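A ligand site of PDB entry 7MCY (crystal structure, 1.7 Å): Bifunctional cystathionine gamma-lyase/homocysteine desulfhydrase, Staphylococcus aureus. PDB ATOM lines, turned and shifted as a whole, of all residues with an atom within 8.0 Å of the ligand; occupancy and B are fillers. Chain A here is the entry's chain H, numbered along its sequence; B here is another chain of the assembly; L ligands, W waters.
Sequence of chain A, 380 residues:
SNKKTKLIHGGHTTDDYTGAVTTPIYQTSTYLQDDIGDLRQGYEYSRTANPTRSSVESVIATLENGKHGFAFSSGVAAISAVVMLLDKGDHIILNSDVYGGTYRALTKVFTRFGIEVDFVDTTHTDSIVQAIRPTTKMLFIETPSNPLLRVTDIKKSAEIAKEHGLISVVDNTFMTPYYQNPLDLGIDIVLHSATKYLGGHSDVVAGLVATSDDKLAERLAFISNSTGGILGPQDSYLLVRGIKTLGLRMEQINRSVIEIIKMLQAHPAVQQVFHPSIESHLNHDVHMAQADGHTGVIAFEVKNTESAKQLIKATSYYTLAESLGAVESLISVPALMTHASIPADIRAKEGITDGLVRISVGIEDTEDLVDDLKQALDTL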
ATOM      1  N   SER A   1     -22.752   0.209   3.234  1.00  0.00           N
ATOM      2  CA  SER A   1     -22.259   0.676   1.939  1.00  0.00           C
ATOM      3  C   SER A   1     -22.549  -0.342   0.834  1.00  0.00           C
ATOM      4  O   SER A   1     -23.677  -0.422   0.361  1.00  0.00           O
ATOM      5  CB  SER A   1     -20.769   0.965   2.015  1.00  0.00           C
ATOM      6  OG  SER A   1     -20.346   1.745   0.904  1.00  0.00           O
ATOM      7  N   ASN A   2     -21.545  -1.109   0.404  1.00  0.00           N
ATOM      8  CA  ASN A   2     -21.784  -2.086  -0.644  1.00  0.00           C
ATOM      9  C   ASN A   2     -22.486  -3.325  -0.073  1.00  0.00           C
ATOM     10  O   ASN A   2     -22.576  -3.517   1.142  1.00  0.00           O
ATOM     11  CB  ASN A   2     -20.476  -2.441  -1.350  1.00  0.00           C
ATOM     12  CG  ASN A   2     -19.959  -1.303  -2.215  1.00  0.00           C
ATOM     13  OD1 ASN A   2     -20.728  -0.505  -2.744  1.00  0.00           O
ATOM     14  ND2 ASN A   2     -18.634  -1.214  -2.362  1.00  0.00           N
ATOM     15  N   LYS A   3     -23.026  -4.163  -0.977  1.00  0.00           N
ATOM     16  CA  LYS A   3     -23.938  -5.230  -0.565  1.00  0.00           C
ATOM     17  C   LYS A   3     -23.275  -6.215   0.407  1.00  0.00           C
ATOM     18  O   LYS A   3     -23.898  -6.668   1.376  1.00  0.00           O
ATOM     19  CB  LYS A   3     -24.459  -5.971  -1.800  1.00  0.00           C
ATOM     20  CG  LYS A   3     -25.152  -5.082  -2.833  1.00  0.00           C
ATOM     21  CD  LYS A   3     -25.938  -5.896  -3.877  1.00  0.00           C
ATOM     22  CE  LYS A   3     -25.003  -6.589  -4.877  1.00  0.00           C
ATOM     23  NZ  LYS A   3     -25.746  -7.256  -6.004  1.00  0.00           N
ATOM     24  N   LYS A   4     -22.025  -6.589   0.134  1.00  0.00           N
ATOM     25  CA  LYS A   4     -21.365  -7.572   0.989  1.00  0.00           C
ATOM     26  C   LYS A   4     -21.123  -7.041   2.389  1.00  0.00           C
ATOM     27  O   LYS A   4     -21.067  -7.809   3.353  1.00  0.00           O
ATOM     28  CB  LYS A   4     -20.052  -8.012   0.345  1.00  0.00           C
ATOM     29  CG  LYS A   4     -20.229  -9.048  -0.747  1.00  0.00           C
ATOM     30  CD  LYS A   4     -18.852  -9.435  -1.278  1.00  0.00           C
ATOM     31  CE  LYS A   4     -18.918 -10.097  -2.617  1.00  0.00           C
ATOM     32  NZ  LYS A   4     -17.587 -10.146  -3.274  1.00  0.00           N
ATOM     33  N   THR A   5     -20.967  -5.725   2.531  1.00  0.00           N
ATOM     34  CA  THR A   5     -20.838  -5.134   3.866  1.00  0.00           C
ATOM     35  C   THR A   5     -22.177  -5.098   4.582  1.00  0.00           C
ATOM     36  O   THR A   5     -22.254  -5.400   5.781  1.00  0.00           O
ATOM     37  CB  THR A   5     -20.259  -3.732   3.731  1.00  0.00           C
ATOM     38  OG1 THR A   5     -19.027  -3.806   3.004  1.00  0.00           O
ATOM     39  CG2 THR A   5     -20.011  -3.100   5.100  1.00  0.00           C
ATOM     40  N   LYS A   6     -23.230  -4.735   3.855  1.00  0.00           N
ATOM     41  CA  LYS A   6     -24.571  -4.690   4.408  1.00  0.00           C
ATOM     42  C   LYS A   6     -25.000  -6.063   4.925  1.00  0.00           C
ATOM     43  O   LYS A   6     -25.705  -6.148   5.937  1.00  0.00           O
ATOM     44  CB  LYS A   6     -25.534  -4.187   3.321  1.00  0.00           C
ATOM     45  CG  LYS A   6     -26.915  -3.807   3.785  1.00  0.00           C
ATOM     46  CD  LYS A   6     -27.655  -3.175   2.606  1.00  0.00           C
ATOM     47  CE  LYS A   6     -29.113  -2.900   2.906  1.00  0.00           C
ATOM     48  NZ  LYS A   6     -29.763  -2.296   1.713  1.00  0.00           N
ATOM     49  N   LEU A   7     -24.571  -7.136   4.265  1.00  0.00           N
ATOM     50  CA  LEU A   7     -24.924  -8.482   4.752  1.00  0.00           C
ATOM     51  C   LEU A   7     -24.316  -8.774   6.116  1.00  0.00           C
ATOM     52  O   LEU A   7     -24.858  -9.586   6.879  1.00  0.00           O
ATOM     53  CB  LEU A   7     -24.458  -9.535   3.754  1.00  0.00           C
ATOM     54  CG  LEU A   7     -25.359  -9.644   2.527  1.00  0.00           C
ATOM     55  CD1 LEU A   7     -24.609 -10.383   1.460  1.00  0.00           C
ATOM     56  CD2 LEU A   7     -26.647 -10.362   2.899  1.00  0.00           C
ATOM     57  N   ILE A   8     -23.178  -8.180   6.418  1.00  0.00           N
ATOM     58  CA  ILE A   8     -22.513  -8.467   7.686  1.00  0.00           C
ATOM     59  C   ILE A   8     -23.005  -7.522   8.778  1.00  0.00           C
ATOM     60  O   ILE A   8     -23.262  -7.941   9.907  1.00  0.00           O
ATOM     61  CB  ILE A   8     -20.994  -8.386   7.507  1.00  0.00           C
ATOM     62  CG1 ILE A   8     -20.534  -9.362   6.417  1.00  0.00           C
ATOM     63  CG2 ILE A   8     -20.269  -8.647   8.830  1.00  0.00           C
ATOM     64  CD1 ILE A   8     -21.052 -10.798   6.599  1.00  0.00           C
ATOM     65  N   HIS A   9     -23.171  -6.251   8.440  1.00  0.00           N
ATOM     66  CA  HIS A   9     -23.450  -5.236   9.451  1.00  0.00           C
ATOM     67  C   HIS A   9     -24.871  -4.715   9.418  1.00  0.00           C
ATOM     68  O   HIS A   9     -25.253  -3.960  10.310  1.00  0.00           O
ATOM     69  CB  HIS A   9     -22.429  -4.099   9.310  1.00  0.00           C
ATOM     70  CG  HIS A   9     -21.017  -4.552   9.526  1.00  0.00           C
ATOM     71  ND1 HIS A   9     -20.531  -4.849  10.782  1.00  0.00           N
ATOM     72  CD2 HIS A   9     -20.022  -4.830   8.656  1.00  0.00           C
ATOM     73  CE1 HIS A   9     -19.278  -5.252  10.683  1.00  0.00           C
ATOM     74  NE2 HIS A   9     -18.949  -5.251   9.404  1.00  0.00           N
ATOM     75  N   GLY A  10     -25.683  -5.121   8.441  1.00  0.00           N
ATOM     76  CA  GLY A  10     -27.080  -4.708   8.417  1.00  0.00           C
ATOM     77  C   GLY A  10     -27.931  -5.476   9.408  1.00  0.00           C
ATOM     78  O   GLY A  10     -27.692  -6.660   9.688  1.00  0.00           O
ATOM     79  N   GLY A  11     -28.949  -4.810   9.933  1.00  0.00           N
ATOM     80  CA  GLY A  11     -29.809  -5.401  10.948  1.00  0.00           C
ATOM     81  C   GLY A  11     -29.116  -5.397  12.296  1.00  0.00           C
ATOM     82  O   GLY A  11     -27.963  -4.991  12.432  1.00  0.00           O
ATOM     83  N   THR A  62     -33.833  -4.890   6.656  1.00  0.00           N
ATOM     84  CA  THR A  62     -32.701  -4.110   6.169  1.00  0.00           C
ATOM     85  C   THR A  62     -32.311  -4.507   4.751  1.00  0.00           C
ATOM     86  O   THR A  62     -32.044  -3.644   3.904  1.00  0.00           O
ATOM     87  CB  THR A  62     -31.502  -4.268   7.111  1.00  0.00           C
ATOM     88  OG1 THR A  62     -31.868  -3.752   8.396  1.00  0.00           O
ATOM     89  CG2 THR A  62     -30.306  -3.505   6.574  1.00  0.00           C
ATOM     90  N   LEU A  63     -32.246  -5.816   4.476  1.00  0.00           N
ATOM     91  CA  LEU A  63     -31.741  -6.275   3.192  1.00  0.00           C
ATOM     92  C   LEU A  63     -32.687  -5.942   2.046  1.00  0.00           C
ATOM     93  O   LEU A  63     -32.245  -5.778   0.909  1.00  0.00           O
ATOM     94  CB  LEU A  63     -31.486  -7.781   3.228  1.00  0.00           C
ATOM     95  CG  LEU A  63     -30.339  -8.200   4.160  1.00  0.00           C
ATOM     96  CD1 LEU A  63     -30.106  -9.692   4.057  1.00  0.00           C
ATOM     97  CD2 LEU A  63     -29.066  -7.417   3.835  1.00  0.00           C
ATOM     98  N   GLU A  64     -33.982  -5.835   2.337  1.00  0.00           N
ATOM     99  CA  GLU A  64     -34.955  -5.492   1.304  1.00  0.00           C
ATOM    100  C   GLU A  64     -35.276  -4.007   1.300  1.00  0.00           C
ATOM    101  O   GLU A  64     -36.196  -3.592   0.585  1.00  0.00           O
ATOM    102  CB  GLU A  64     -36.230  -6.328   1.479  1.00  0.00           C
ATOM    103  CG  GLU A  64     -36.074  -7.812   1.106  1.00  0.00           C
ATOM    104  CD  GLU A  64     -35.959  -8.083  -0.406  1.00  0.00           C
ATOM    105  OE1 GLU A  64     -35.648  -7.151  -1.186  1.00  0.00           O
ATOM    106  OE2 GLU A  64     -36.184  -9.239  -0.823  1.00  0.00           O
ATOM    107  N   ASN A  65     -34.543  -3.196   2.065  1.00  0.00           N
ATOM    108  CA  ASN A  65     -34.796  -1.754   2.160  1.00  0.00           C
ATOM    109  C   ASN A  65     -36.236  -1.468   2.598  1.00  0.00           C
ATOM    110  O   ASN A  65     -36.885  -0.542   2.102  1.00  0.00           O
ATOM    111  CB  ASN A  65     -34.468  -1.050   0.843  1.00  0.00           C
ATOM    112  CG  ASN A  65     -33.010  -1.176   0.481  1.00  0.00           C
ATOM    113  OD1 ASN A  65     -32.145  -1.191   1.347  1.00  0.00           O
ATOM    114  ND2 ASN A  65     -32.731  -1.286  -0.826  1.00  0.00           N
ATOM    115  N   ASN A 181     -34.636  -6.149  -5.464  1.00  0.00           N
ATOM    116  CA  ASN A 181     -35.251  -5.501  -4.299  1.00  0.00           C
ATOM    117  C   ASN A 181     -36.591  -4.918  -4.695  1.00  0.00           C
ATOM    118  O   ASN A 181     -36.686  -3.724  -5.010  1.00  0.00           O
ATOM    119  CB  ASN A 181     -34.335  -4.437  -3.715  1.00  0.00           C
ATOM    120  CG  ASN A 181     -33.005  -5.000  -3.262  1.00  0.00           C
ATOM    121  OD1 ASN A 181     -31.938  -4.586  -3.719  1.00  0.00           O
ATOM    122  ND2 ASN A 181     -33.061  -5.971  -2.342  1.00  0.00           N
ATOM    123  N   ASP A 184     -37.974  -1.462  -3.502  1.00  0.00           N
ATOM    124  CA  ASP A 184     -37.386  -0.285  -4.131  1.00  0.00           C
ATOM    125  C   ASP A 184     -38.085   0.074  -5.430  1.00  0.00           C
ATOM    126  O   ASP A 184     -37.977   1.209  -5.900  1.00  0.00           O
ATOM    127  CB  ASP A 184     -35.907  -0.509  -4.422  1.00  0.00           C
ATOM    128  CG  ASP A 184     -35.053  -0.435  -3.186  1.00  0.00           C
ATOM    129  OD1 ASP A 184     -35.543   0.031  -2.128  1.00  0.00           O
ATOM    130  OD2 ASP A 184     -33.869  -0.818  -3.272  1.00  0.00           O
ATOM    131  N   SER B 316     -15.656   2.301  10.797  1.00  0.00           N
ATOM    132  CA  SER B 316     -17.042   1.877  10.860  1.00  0.00           C
ATOM    133  C   SER B 316     -17.225   0.370  10.789  1.00  0.00           C
ATOM    134  O   SER B 316     -18.174  -0.156  11.368  1.00  0.00           O
ATOM    135  CB  SER B 316     -17.846   2.514   9.725  1.00  0.00           C
ATOM    136  OG  SER B 316     -17.989   3.909   9.924  1.00  0.00           O
ATOM    137  N   TYR B 317     -16.323  -0.332  10.101  1.00  0.00           N
ATOM    138  CA  TYR B 317     -16.527  -1.740   9.764  1.00  0.00           C
ATOM    139  C   TYR B 317     -15.527  -2.669  10.429  1.00  0.00           C
ATOM    140  O   TYR B 317     -15.511  -3.859  10.110  1.00  0.00           O
ATOM    141  CB  TYR B 317     -16.469  -1.915   8.238  1.00  0.00           C
ATOM    142  CG  TYR B 317     -17.459  -1.040   7.519  1.00  0.00           C
ATOM    143  CD1 TYR B 317     -18.786  -0.987   7.924  1.00  0.00           C
ATOM    144  CD2 TYR B 317     -17.069  -0.248   6.437  1.00  0.00           C
ATOM    145  CE1 TYR B 317     -19.712  -0.185   7.271  1.00  0.00           C
ATOM    146  CE2 TYR B 317     -17.991   0.575   5.787  1.00  0.00           C
ATOM    147  CZ  TYR B 317     -19.311   0.597   6.209  1.00  0.00           C
ATOM    148  OH  TYR B 317     -20.238   1.394   5.579  1.00  0.00           O
ATOM    149  N   GLU B 364     -16.580  -8.576   4.502  1.00  0.00           N
ATOM    150  CA  GLU B 364     -17.241  -7.382   3.989  1.00  0.00           C
ATOM    151  C   GLU B 364     -16.688  -7.022   2.601  1.00  0.00           C
ATOM    152  O   GLU B 364     -15.677  -7.556   2.142  1.00  0.00           O
ATOM    153  CB  GLU B 364     -17.063  -6.215   4.957  1.00  0.00           C
ATOM    154  CG  GLU B 364     -17.617  -6.470   6.358  1.00  0.00           C
ATOM    155  CD  GLU B 364     -16.548  -6.907   7.351  1.00  0.00           C
ATOM    156  OE1 GLU B 364     -15.549  -7.530   6.915  1.00  0.00           O
ATOM    157  OE2 GLU B 364     -16.704  -6.630   8.560  1.00  0.00           O
ATOM    158  N   ASP B 368     -15.096  -1.306   0.668  1.00  0.00           N
ATOM    159  CA  ASP B 368     -15.503  -0.710   1.939  1.00  0.00           C
ATOM    160  C   ASP B 368     -14.427  -0.874   3.001  1.00  0.00           C
ATOM    161  O   ASP B 368     -14.144   0.055   3.753  1.00  0.00           O
ATOM    162  CB  ASP B 368     -16.807  -1.321   2.431  1.00  0.00           C
ATOM    163  CG  ASP B 368     -18.010  -0.882   1.607  1.00  0.00           C
ATOM    164  OD1 ASP B 368     -17.931   0.194   0.969  1.00  0.00           O
ATOM    165  OD2 ASP B 368     -19.006  -1.625   1.600  1.00  0.00           O
HETATM  166  N1  LIG L   1     -26.724  -0.842   6.365  1.00  0.00           N
HETATM  167  C1  LIG L   1     -25.424  -1.150   6.389  1.00  0.00           C
HETATM  168  C2  LIG L   1     -24.904  -1.955   7.554  1.00  0.00           C
HETATM  169  C3  LIG L   1     -24.570  -0.743   5.383  1.00  0.00           C
HETATM  170  O1  LIG L   1     -23.251  -1.080   5.449  1.00  0.00           O
HETATM  171  C4  LIG L   1     -25.055   0.008   4.310  1.00  0.00           C
HETATM  172  C5  LIG L   1     -24.161   0.450   3.212  1.00  0.00           C
HETATM  173  C6  LIG L   1     -26.442   0.327   4.284  1.00  0.00           C
HETATM  174  C7  LIG L   1     -27.215  -0.120   5.337  1.00  0.00           C
HETATM  175  C8  LIG L   1     -27.078   1.140   3.179  1.00  0.00           C
HETATM  176  O2  LIG L   1     -27.523   0.260   2.144  1.00  0.00           O
HETATM  177  P1  LIG L   1     -28.129   0.810   0.751  1.00  0.00           P
HETATM  178  O3  LIG L   1     -29.532   1.344   0.981  1.00  0.00           O
HETATM  179  O4  LIG L   1     -27.245   1.911   0.223  1.00  0.00           O
HETATM  180  O5  LIG L   1     -28.173  -0.348  -0.232  1.00  0.00           O
HETATM  181  O   HOH W   1     -25.819  -1.757  -0.568  1.00  0.00           O
HETATM  182  O   HOH W   2     -24.747   1.685  -1.026  1.00  0.00           O
HETATM  183  O   HOH W   3     -29.928  -1.528  -1.790  1.00  0.00           O
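The backbone NH (N) of Ser 1 is bonded to a carbon (C5) of the ligand (1.4 Å). The side-chain amino group (NZ) of Lys 6 lies within salt-bridge range of an oxygen (O5) of the ligand.
Water W3 bridges O5 of the ligand (2.6 Å) and ND2 of Asn 65 (3.0 Å). Water W1 lies within hydrogen-bond range of the backbone carbonyl oxygen (O) of Ser 1 (2.7 Å) and an oxygen (O5) of the ligand (2.8 Å). Water W2 bridges the backbone carbonyl oxygen (O) of Ser 1 (2.7 Å) and an oxygen (O4) of the ligand (2.8 Å).
Merely in contact with the ligand: Thr 5 (3.8 Å), His 9 (3.3 Å), Gly 10 (3.4 Å), Asn 65 (3.7 Å) and Tyr 317 of chain B (3.9 Å). Hydrophobic or aromatic side chains that line the ligand: His 9. The nearest printed residue that does not touch the ligand is Asn 2 (4.1 Å).
The side-chain hydroxyl (OG) of Ser 1 sits at hydrogen-bond distance from the side-chain carboxylate (OD1) of Asp 368 of chain B, at 2.9 Å. The side-chain amide oxygen (OD1) of Asn 65 lies within hydrogen-bond range of the side-chain amino group (NZ) of Lys 6 (2.7 Å). The side-chain amino group (NZ) of Lys 6 sits close to the backbone carbonyl oxygen (O) of Thr 62 (3.4 Å). The side-chain carboxylate (OE2) of Glu 364 of chain B is in hydrogen-bond range of a ring nitrogen (NE2) of His 9 (2.8 Å). The side-chain carboxylate (OD2) of Asp 184 is in hydrogen-bond range of the side-chain amide nitrogen (ND2) of Asn 65. The side-chain carboxylate (OD2) of Asp 368 of chain B sits at hydrogen-bond distance from the side-chain hydroxyl (OG1) of Thr 5, at 2.6 Å.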
